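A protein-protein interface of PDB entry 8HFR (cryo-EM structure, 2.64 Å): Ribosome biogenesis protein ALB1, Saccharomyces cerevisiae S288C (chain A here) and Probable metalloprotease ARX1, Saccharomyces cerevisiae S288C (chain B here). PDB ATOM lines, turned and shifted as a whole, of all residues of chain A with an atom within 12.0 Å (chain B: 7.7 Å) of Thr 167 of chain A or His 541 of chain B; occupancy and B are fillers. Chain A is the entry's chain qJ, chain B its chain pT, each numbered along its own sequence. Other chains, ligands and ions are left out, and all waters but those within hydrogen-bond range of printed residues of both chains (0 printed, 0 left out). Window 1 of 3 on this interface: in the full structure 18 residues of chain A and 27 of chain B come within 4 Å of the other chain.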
ATOM      1  N   GLY A 164       2.880   5.993   8.754  1.00  0.00           N
ATOM      2  CA  GLY A 164       2.849   5.970  10.205  1.00  0.00           C
ATOM      3  C   GLY A 164       3.699   7.062  10.809  1.00  0.00           C
ATOM      4  O   GLY A 164       4.545   6.789  11.659  1.00  0.00           O
ATOM      5  N   GLN A 165       3.484   8.282  10.312  1.00  0.00           N
ATOM      6  CA  GLN A 165       4.096   9.564  10.678  1.00  0.00           C
ATOM      7  C   GLN A 165       5.548   9.714  10.230  1.00  0.00           C
ATOM      8  O   GLN A 165       6.069  10.835  10.291  1.00  0.00           O
ATOM      9  CB  GLN A 165       4.022   9.863  12.183  1.00  0.00           C
ATOM     10  CG  GLN A 165       2.815  10.672  12.586  1.00  0.00           C
ATOM     11  CD  GLN A 165       2.746  11.989  11.851  1.00  0.00           C
ATOM     12  OE1 GLN A 165       1.738  12.312  11.225  1.00  0.00           O
ATOM     13  NE2 GLN A 165       3.826  12.753  11.912  1.00  0.00           N
ATOM     14  N   GLY A 166       6.193   8.653   9.737  1.00  0.00           N
ATOM     15  CA  GLY A 166       7.566   8.665   9.265  1.00  0.00           C
ATOM     16  C   GLY A 166       8.596   9.239  10.214  1.00  0.00           C
ATOM     17  O   GLY A 166       8.456   9.118  11.433  1.00  0.00           O
ATOM     18  N   THR A 167       9.628   9.871   9.660  1.00  0.00           N
ATOM     19  CA  THR A 167      10.543  10.699  10.431  1.00  0.00           C
ATOM     20  C   THR A 167      10.830  11.968   9.650  1.00  0.00           C
ATOM     21  O   THR A 167      10.573  12.051   8.447  1.00  0.00           O
ATOM     22  CB  THR A 167      11.856   9.980  10.763  1.00  0.00           C
ATOM     23  OG1 THR A 167      12.256   9.146   9.667  1.00  0.00           O
ATOM     24  CG2 THR A 167      11.709   9.152  12.025  1.00  0.00           C
ATOM     25  N   THR A 168      11.362  12.963  10.352  1.00  0.00           N
ATOM     26  CA  THR A 168      11.727  14.228   9.733  1.00  0.00           C
ATOM     27  C   THR A 168      12.858  14.868  10.530  1.00  0.00           C
ATOM     28  O   THR A 168      12.917  14.738  11.755  1.00  0.00           O
ATOM     29  CB  THR A 168      10.516  15.169   9.625  1.00  0.00           C
ATOM     30  OG1 THR A 168      10.929  16.444   9.119  1.00  0.00           O
ATOM     31  CG2 THR A 168       9.818  15.340  10.963  1.00  0.00           C
ATOM     32  N   LEU A 169      13.778  15.514   9.816  1.00  0.00           N
ATOM     33  CA  LEU A 169      14.874  16.259  10.421  1.00  0.00           C
ATOM     34  C   LEU A 169      15.069  17.549   9.645  1.00  0.00           C
ATOM     35  O   LEU A 169      14.788  17.616   8.447  1.00  0.00           O
ATOM     36  CB  LEU A 169      16.195  15.472  10.432  1.00  0.00           C
ATOM     37  CG  LEU A 169      16.250  14.005  10.868  1.00  0.00           C
ATOM     38  CD1 LEU A 169      17.525  13.351  10.368  1.00  0.00           C
ATOM     39  CD2 LEU A 169      16.139  13.874  12.370  1.00  0.00           C
ATOM     40  N   GLY A 170      15.540  18.582  10.341  1.00  0.00           N
ATOM     41  CA  GLY A 170      15.783  19.868   9.717  1.00  0.00           C
ATOM     42  C   GLY A 170      14.527  20.662   9.429  1.00  0.00           C
ATOM     43  O   GLY A 170      13.416  20.131   9.498  1.00  0.00           O
ATOM     44  N   GLY A 171      14.681  21.939   9.102  1.00  0.00           N
ATOM     45  CA  GLY A 171      13.542  22.801   8.906  1.00  0.00           C
ATOM     46  C   GLY A 171      13.601  23.571   7.606  1.00  0.00           C
ATOM     47  O   GLY A 171      14.451  23.321   6.749  1.00  0.00           O
ATOM     48  N   LEU B 176      13.469  16.989   1.220  1.00  0.00           N
ATOM     49  CA  LEU B 176      13.928  15.943   0.325  1.00  0.00           C
ATOM     50  C   LEU B 176      13.310  14.627   0.760  1.00  0.00           C
ATOM     51  O   LEU B 176      13.311  14.300   1.951  1.00  0.00           O
ATOM     52  CB  LEU B 176      15.449  15.850   0.347  1.00  0.00           C
ATOM     53  CG  LEU B 176      16.067  14.852  -0.621  1.00  0.00           C
ATOM     54  CD1 LEU B 176      16.219  15.482  -1.993  1.00  0.00           C
ATOM     55  CD2 LEU B 176      17.394  14.372  -0.088  1.00  0.00           C
ATOM     56  N   GLY B 178      12.726  10.333  -0.326  1.00  0.00           N
ATOM     57  CA  GLY B 178      13.156   9.185  -1.089  1.00  0.00           C
ATOM     58  C   GLY B 178      14.309   8.476  -0.406  1.00  0.00           C
ATOM     59  O   GLY B 178      14.506   8.584   0.813  1.00  0.00           O
ATOM     60  N   GLY B 179      15.080   7.747  -1.214  1.00  0.00           N
ATOM     61  CA  GLY B 179      16.159   6.945  -0.670  1.00  0.00           C
ATOM     62  C   GLY B 179      17.317   7.777  -0.164  1.00  0.00           C
ATOM     63  O   GLY B 179      18.022   7.377   0.767  1.00  0.00           O
ATOM     64  N   ALA B 181      16.822  10.604   1.354  1.00  0.00           N
ATOM     65  CA  ALA B 181      16.336  10.990   2.673  1.00  0.00           C
ATOM     66  C   ALA B 181      16.506   9.859   3.677  1.00  0.00           C
ATOM     67  O   ALA B 181      16.861  10.102   4.839  1.00  0.00           O
ATOM     68  CB  ALA B 181      14.877  11.416   2.584  1.00  0.00           C
ATOM     69  N   ASP B 182      16.284   8.615   3.239  1.00  0.00           N
ATOM     70  CA  ASP B 182      16.505   7.462   4.112  1.00  0.00           C
ATOM     71  C   ASP B 182      17.972   7.334   4.513  1.00  0.00           C
ATOM     72  O   ASP B 182      18.285   7.072   5.681  1.00  0.00           O
ATOM     73  CB  ASP B 182      16.037   6.182   3.426  1.00  0.00           C
ATOM     74  CG  ASP B 182      14.622   6.276   2.929  1.00  0.00           C
ATOM     75  OD1 ASP B 182      13.799   6.930   3.600  1.00  0.00           O
ATOM     76  OD2 ASP B 182      14.331   5.707   1.857  1.00  0.00           O
ATOM     77  N   ALA B 183      18.883   7.541   3.559  1.00  0.00           N
ATOM     78  CA  ALA B 183      20.310   7.424   3.851  1.00  0.00           C
ATOM     79  C   ALA B 183      20.788   8.542   4.764  1.00  0.00           C
ATOM     80  O   ALA B 183      21.593   8.302   5.673  1.00  0.00           O
ATOM     81  CB  ALA B 183      21.115   7.411   2.553  1.00  0.00           C
ATOM     82  N   ALA B 185      18.927  10.201   6.982  1.00  0.00           N
ATOM     83  CA  ALA B 185      18.366   9.953   8.307  1.00  0.00           C
ATOM     84  C   ALA B 185      19.113   8.843   9.035  1.00  0.00           C
ATOM     85  O   ALA B 185      19.435   8.978  10.222  1.00  0.00           O
ATOM     86  CB  ALA B 185      16.884   9.608   8.186  1.00  0.00           C
ATOM     87  N   ALA B 186      19.421   7.750   8.325  1.00  0.00           N
ATOM     88  CA  ALA B 186      20.131   6.634   8.943  1.00  0.00           C
ATOM     89  C   ALA B 186      21.544   7.022   9.362  1.00  0.00           C
ATOM     90  O   ALA B 186      21.991   6.650  10.455  1.00  0.00           O
ATOM     91  CB  ALA B 186      20.165   5.443   7.988  1.00  0.00           C
ATOM     92  N   ILE B 189      21.308   9.420  12.503  1.00  0.00           N
ATOM     93  CA  ILE B 189      20.826   8.750  13.706  1.00  0.00           C
ATOM     94  C   ILE B 189      21.868   7.768  14.242  1.00  0.00           C
ATOM     95  O   ILE B 189      22.106   7.702  15.460  1.00  0.00           O
ATOM     96  CB  ILE B 189      19.469   8.082  13.409  1.00  0.00           C
ATOM     97  CG1 ILE B 189      18.363   9.126  13.496  1.00  0.00           C
ATOM     98  CG2 ILE B 189      19.162   6.952  14.366  1.00  0.00           C
ATOM     99  CD1 ILE B 189      17.169   8.825  12.658  1.00  0.00           C
ATOM    100  N   ALA B 231      20.359   0.685  10.420  1.00  0.00           N
ATOM    101  CA  ALA B 231      20.388   0.551   8.964  1.00  0.00           C
ATOM    102  C   ALA B 231      19.216  -0.279   8.443  1.00  0.00           C
ATOM    103  O   ALA B 231      18.565   0.097   7.460  1.00  0.00           O
ATOM    104  CB  ALA B 231      21.716  -0.061   8.531  1.00  0.00           C
ATOM    105  N   ARG B 232      18.920  -1.406   9.098  1.00  0.00           N
ATOM    106  CA  ARG B 232      17.795  -2.227   8.662  1.00  0.00           C
ATOM    107  C   ARG B 232      16.459  -1.565   8.971  1.00  0.00           C
ATOM    108  O   ARG B 232      15.462  -1.849   8.301  1.00  0.00           O
ATOM    109  CB  ARG B 232      17.861  -3.608   9.313  1.00  0.00           C
ATOM    110  N   SER B 233      16.416  -0.681   9.972  1.00  0.00           N
ATOM    111  CA  SER B 233      15.190   0.062  10.233  1.00  0.00           C
ATOM    112  C   SER B 233      14.925   1.081   9.142  1.00  0.00           C
ATOM    113  O   SER B 233      13.770   1.314   8.769  1.00  0.00           O
ATOM    114  CB  SER B 233      15.271   0.749  11.591  1.00  0.00           C
ATOM    115  OG  SER B 233      15.455  -0.202  12.620  1.00  0.00           O
ATOM    116  N   TYR B 234      15.976   1.701   8.610  1.00  0.00           N
ATOM    117  CA  TYR B 234      15.782   2.724   7.589  1.00  0.00           C
ATOM    118  C   TYR B 234      15.989   2.230   6.168  1.00  0.00           C
ATOM    119  O   TYR B 234      16.008   3.060   5.254  1.00  0.00           O
ATOM    120  CB  TYR B 234      16.691   3.910   7.850  1.00  0.00           C
ATOM    121  CG  TYR B 234      16.093   4.837   8.849  1.00  0.00           C
ATOM    122  CD1 TYR B 234      15.183   5.804   8.460  1.00  0.00           C
ATOM    123  CD2 TYR B 234      16.408   4.726  10.186  1.00  0.00           C
ATOM    124  CE1 TYR B 234      14.622   6.642   9.374  1.00  0.00           C
ATOM    125  CE2 TYR B 234      15.858   5.556  11.098  1.00  0.00           C
ATOM    126  CZ  TYR B 234      14.963   6.510  10.694  1.00  0.00           C
ATOM    127  OH  TYR B 234      14.409   7.340  11.626  1.00  0.00           O
ATOM    128  N   ASN B 235      16.149   0.915   5.968  1.00  0.00           N
ATOM    129  CA  ASN B 235      16.281   0.280   4.648  1.00  0.00           C
ATOM    130  C   ASN B 235      17.494   0.829   3.890  1.00  0.00           C
ATOM    131  O   ASN B 235      17.386   1.492   2.858  1.00  0.00           O
ATOM    132  CB  ASN B 235      14.985   0.414   3.835  1.00  0.00           C
ATOM    133  CG  ASN B 235      15.012  -0.379   2.544  1.00  0.00           C
ATOM    134  OD1 ASN B 235      15.746  -1.355   2.416  1.00  0.00           O
ATOM    135  ND2 ASN B 235      14.216   0.052   1.574  1.00  0.00           N
ATOM    136  N   CYS B 236      18.664   0.569   4.455  1.00  0.00           N
ATOM    137  CA  CYS B 236      19.915   1.042   3.890  1.00  0.00           C
ATOM    138  C   CYS B 236      20.988   0.002   4.144  1.00  0.00           C
ATOM    139  O   CYS B 236      20.844  -0.871   5.000  1.00  0.00           O
ATOM    140  CB  CYS B 236      20.332   2.389   4.488  1.00  0.00           C
ATOM    141  SG  CYS B 236      19.638   3.806   3.648  1.00  0.00           S
ATOM    142  N   GLU B 327      16.577   1.480  -2.113  1.00  0.00           N
ATOM    143  CA  GLU B 327      15.142   1.480  -2.381  1.00  0.00           C
ATOM    144  C   GLU B 327      14.820   0.913  -3.756  1.00  0.00           C
ATOM    145  O   GLU B 327      13.732   0.370  -3.968  1.00  0.00           O
ATOM    146  CB  GLU B 327      14.591   2.897  -2.253  1.00  0.00           C
ATOM    147  CG  GLU B 327      13.101   2.947  -1.968  1.00  0.00           C
ATOM    148  CD  GLU B 327      12.444   4.206  -2.491  1.00  0.00           C
ATOM    149  OE1 GLU B 327      13.115   4.989  -3.191  1.00  0.00           O
ATOM    150  OE2 GLU B 327      11.245   4.402  -2.209  1.00  0.00           O
ATOM    151  N   ILE B 537      14.733  16.956   5.453  1.00  0.00           N
ATOM    152  CA  ILE B 537      14.324  15.695   4.850  1.00  0.00           C
ATOM    153  C   ILE B 537      13.057  15.210   5.537  1.00  0.00           C
ATOM    154  O   ILE B 537      12.705  15.649   6.632  1.00  0.00           O
ATOM    155  CB  ILE B 537      15.407  14.600   4.947  1.00  0.00           C
ATOM    156  CG1 ILE B 537      15.644  14.230   6.405  1.00  0.00           C
ATOM    157  CG2 ILE B 537      16.705  15.029   4.285  1.00  0.00           C
ATOM    158  CD1 ILE B 537      16.334  12.932   6.582  1.00  0.00           C
ATOM    159  N   HIS B 538      12.373  14.285   4.872  1.00  0.00           N
ATOM    160  CA  HIS B 538      11.280  13.532   5.473  1.00  0.00           C
ATOM    161  C   HIS B 538      11.291  12.131   4.889  1.00  0.00           C
ATOM    162  O   HIS B 538      11.280  11.964   3.667  1.00  0.00           O
ATOM    163  CB  HIS B 538       9.924  14.203   5.233  1.00  0.00           C
ATOM    164  CG  HIS B 538       8.757  13.284   5.423  1.00  0.00           C
ATOM    165  ND1 HIS B 538       8.309  12.899   6.668  1.00  0.00           N
ATOM    166  CD2 HIS B 538       7.951  12.667   4.525  1.00  0.00           C
ATOM    167  CE1 HIS B 538       7.276  12.085   6.529  1.00  0.00           C
ATOM    168  NE2 HIS B 538       7.040  11.929   5.239  1.00  0.00           N
ATOM    169  N   SER B 539      11.321  11.128   5.757  1.00  0.00           N
ATOM    170  CA  SER B 539      11.375   9.736   5.345  1.00  0.00           C
ATOM    171  C   SER B 539      10.090   9.025   5.743  1.00  0.00           C
ATOM    172  O   SER B 539       9.367   9.465   6.637  1.00  0.00           O
ATOM    173  CB  SER B 539      12.564   9.024   5.967  1.00  0.00           C
ATOM    174  OG  SER B 539      12.488   7.636   5.723  1.00  0.00           O
ATOM    175  N   GLN B 540       9.810   7.919   5.056  1.00  0.00           N
ATOM    176  CA  GLN B 540       8.634   7.123   5.373  1.00  0.00           C
ATOM    177  C   GLN B 540       8.911   6.120   6.483  1.00  0.00           C
ATOM    178  O   GLN B 540       8.009   5.805   7.265  1.00  0.00           O
ATOM    179  CB  GLN B 540       8.146   6.392   4.125  1.00  0.00           C
ATOM    180  CG  GLN B 540       7.963   7.288   2.915  1.00  0.00           C
ATOM    181  CD  GLN B 540       6.678   8.091   2.958  1.00  0.00           C
ATOM    182  OE1 GLN B 540       6.698   9.300   3.176  1.00  0.00           O
ATOM    183  NE2 GLN B 540       5.555   7.424   2.736  1.00  0.00           N
ATOM    184  N   HIS B 541      10.134   5.614   6.570  1.00  0.00           N
ATOM    185  CA  HIS B 541      10.499   4.647   7.591  1.00  0.00           C
ATOM    186  C   HIS B 541      10.814   5.344   8.909  1.00  0.00           C
ATOM    187  O   HIS B 541      10.967   6.566   8.975  1.00  0.00           O
ATOM    188  CB  HIS B 541      11.701   3.815   7.144  1.00  0.00           C
ATOM    189  CG  HIS B 541      11.599   3.325   5.736  1.00  0.00           C
ATOM    190  ND1 HIS B 541      12.478   3.708   4.749  1.00  0.00           N
ATOM    191  CD2 HIS B 541      10.710   2.492   5.147  1.00  0.00           C
ATOM    192  CE1 HIS B 541      12.141   3.126   3.613  1.00  0.00           C
ATOM    193  NE2 HIS B 541      11.071   2.385   3.827  1.00  0.00           N
ATOM    194  N   GLU B 542      10.932   4.533   9.959  1.00  0.00           N
ATOM    195  CA  GLU B 542      11.142   5.008  11.322  1.00  0.00           C
ATOM    196  C   GLU B 542      11.595   3.830  12.173  1.00  0.00           C
ATOM    197  O   GLU B 542      11.536   2.677  11.747  1.00  0.00           O
ATOM    198  CB  GLU B 542       9.867   5.658  11.862  1.00  0.00           C
ATOM    199  CG  GLU B 542       8.638   4.785  11.703  1.00  0.00           C
ATOM    200  CD  GLU B 542       8.295   4.026  12.948  1.00  0.00           C
ATOM    201  OE1 GLU B 542       8.662   4.505  14.033  1.00  0.00           O
ATOM    202  OE2 GLU B 542       7.660   2.958  12.849  1.00  0.00           O
ATOM    203  N   LEU B 543      12.057   4.133  13.387  1.00  0.00           N
ATOM    204  CA  LEU B 543      12.464   3.091  14.321  1.00  0.00           C
ATOM    205  C   LEU B 543      11.237   2.429  14.930  1.00  0.00           C
ATOM    206  O   LEU B 543      10.472   3.075  15.649  1.00  0.00           O
ATOM    207  CB  LEU B 543      13.330   3.654  15.448  1.00  0.00           C
ATOM    208  CG  LEU B 543      14.826   3.971  15.356  1.00  0.00           C
ATOM    209  CD1 LEU B 543      15.639   2.789  14.861  1.00  0.00           C
ATOM    210  CD2 LEU B 543      15.100   5.221  14.557  1.00  0.00           C
ATOM    211  N   ASN B 544      11.068   1.144  14.669  1.00  0.00           N
ATOM    212  CA  ASN B 544       9.985   0.372  15.271  1.00  0.00           C
ATOM    213  C   ASN B 544      10.201   0.234  16.771  1.00  0.00           C
ATOM    214  O   ASN B 544      11.190  -0.381  17.186  1.00  0.00           O
ATOM    215  CB  ASN B 544       9.912  -1.007  14.638  1.00  0.00           C
ATOM    216  CG  ASN B 544       8.684  -1.768  15.047  1.00  0.00           C
ATOM    217  OD1 ASN B 544       7.666  -1.180  15.403  1.00  0.00           O
ATOM    218  ND2 ASN B 544       8.771  -3.090  15.018  1.00  0.00           N
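The side-chain hydroxyl (OG1) of Thr 167 of chain A lies close to the side-chain hydroxyl (OH) of Tyr 234 of chain B (3.4 Å).
A ring nitrogen (ND1) of His 538 of chain B lies within hydrogen-bond range of the backbone carbonyl oxygen of Thr 167 of chain A, at 3.0 Å.
O of Thr 167 of chain A is in hydrogen-bond range of N of Ser 539 of chain B (2.9 Å).
OG1 of Thr 167 of chain A lies within hydrogen-bond range of O of His 541 of chain B, 3.0 Å away.
O of Ile 537 of chain B lies within hydrogen-bond range of OG1 of Thr 168 of chain A, at 3.2 Å.
The backbone NH (N) of Ile 537 of chain B lies within hydrogen-bond range of the backbone carbonyl oxygen (O) of Leu 169 of chain A, 3.1 Å away.
The backbone NH (N) of His 538 of chain B is in hydrogen-bond range of the backbone carbonyl oxygen (O) of Leu 176 of chain B, at 3.1 Å.
The side-chain hydroxyl (OG) of Ser 539 of chain B sits at hydrogen-bond distance from the side-chain carboxylate (OD1) of Asp 182 of chain B (2.6 Å).
A ring nitrogen (NE2) of His 538 of chain B is in hydrogen-bond range of the side-chain amide oxygen of Gln 540 of chain B (3.4 Å).
The side-chain hydroxyl (OG) of Ser 539 of chain B lies within hydrogen-bond range of the backbone NH (N) of His 541 of chain B (3.2 Å).
Gly 166 of chain A touches Ser 539 of chain B.
O of Gln 540 of chain B touches CA of Gly 166 of chain A (3.5 Å).
Gly 166 of chain A touches His 541 of chain B (C to O, 3.8 Å).
Gly 166 of chain A touches Glu 542 of chain B.
Thr 167 of chain A touches Glu 542 of chain B.
Thr 167 of chain A touches just these residues of chain B: Tyr 234, His 538, Ser 539, His 541 and Glu 542.
His 541 of chain B touches just these residues of chain A: Gly 166 (3.8 Å) and Thr 167 (3.0 Å).
Of the printed residues of chain B, Gly 166 of chain A touches Ser 539 (3.3 Å), Gln 540 (3.5 Å), His 541 (3.8 Å) and Glu 542 (3.8 Å).
No residue of chain A comes within 4 Å of Gly 179 of chain B.
No residue of chain A comes within 4 Å of Asp 182 of chain B.
Ala 185 of chain B touches none of the printed residues of chain A.
Of chain A, only Thr 167 (3.3 Å) comes within 4 Å of Tyr 234 of chain B.
Printed residues of chain A within 4 Å of His 538 of chain B: Thr 167.
Printed residues of chain A within 4 Å of Ile 537 of chain B: Thr 168 (3.2 Å) and Leu 169 (3.1 Å).
Printed residues of chain B within 4 Å of Leu 169 of chain A: Ile 537.
Of the printed residues of chain B, Thr 168 of chain A touches Ile 537 (3.2 Å).
The nearest printed residue of chain B that does not touch Thr 168 of chain A is His 538 of chain B (4.3 Å).
Of the 8 printed residues of chain A, 4 touch a printed residue of chain B.
Hydrophobic or aromatic side chains of chain A within 4 Å of the printed part of chain B: Leu 169.
Among the printed residues, no Asp or Glu carboxylate lies within 4 Å of a Lys or Arg side-chain nitrogen of the other chain.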
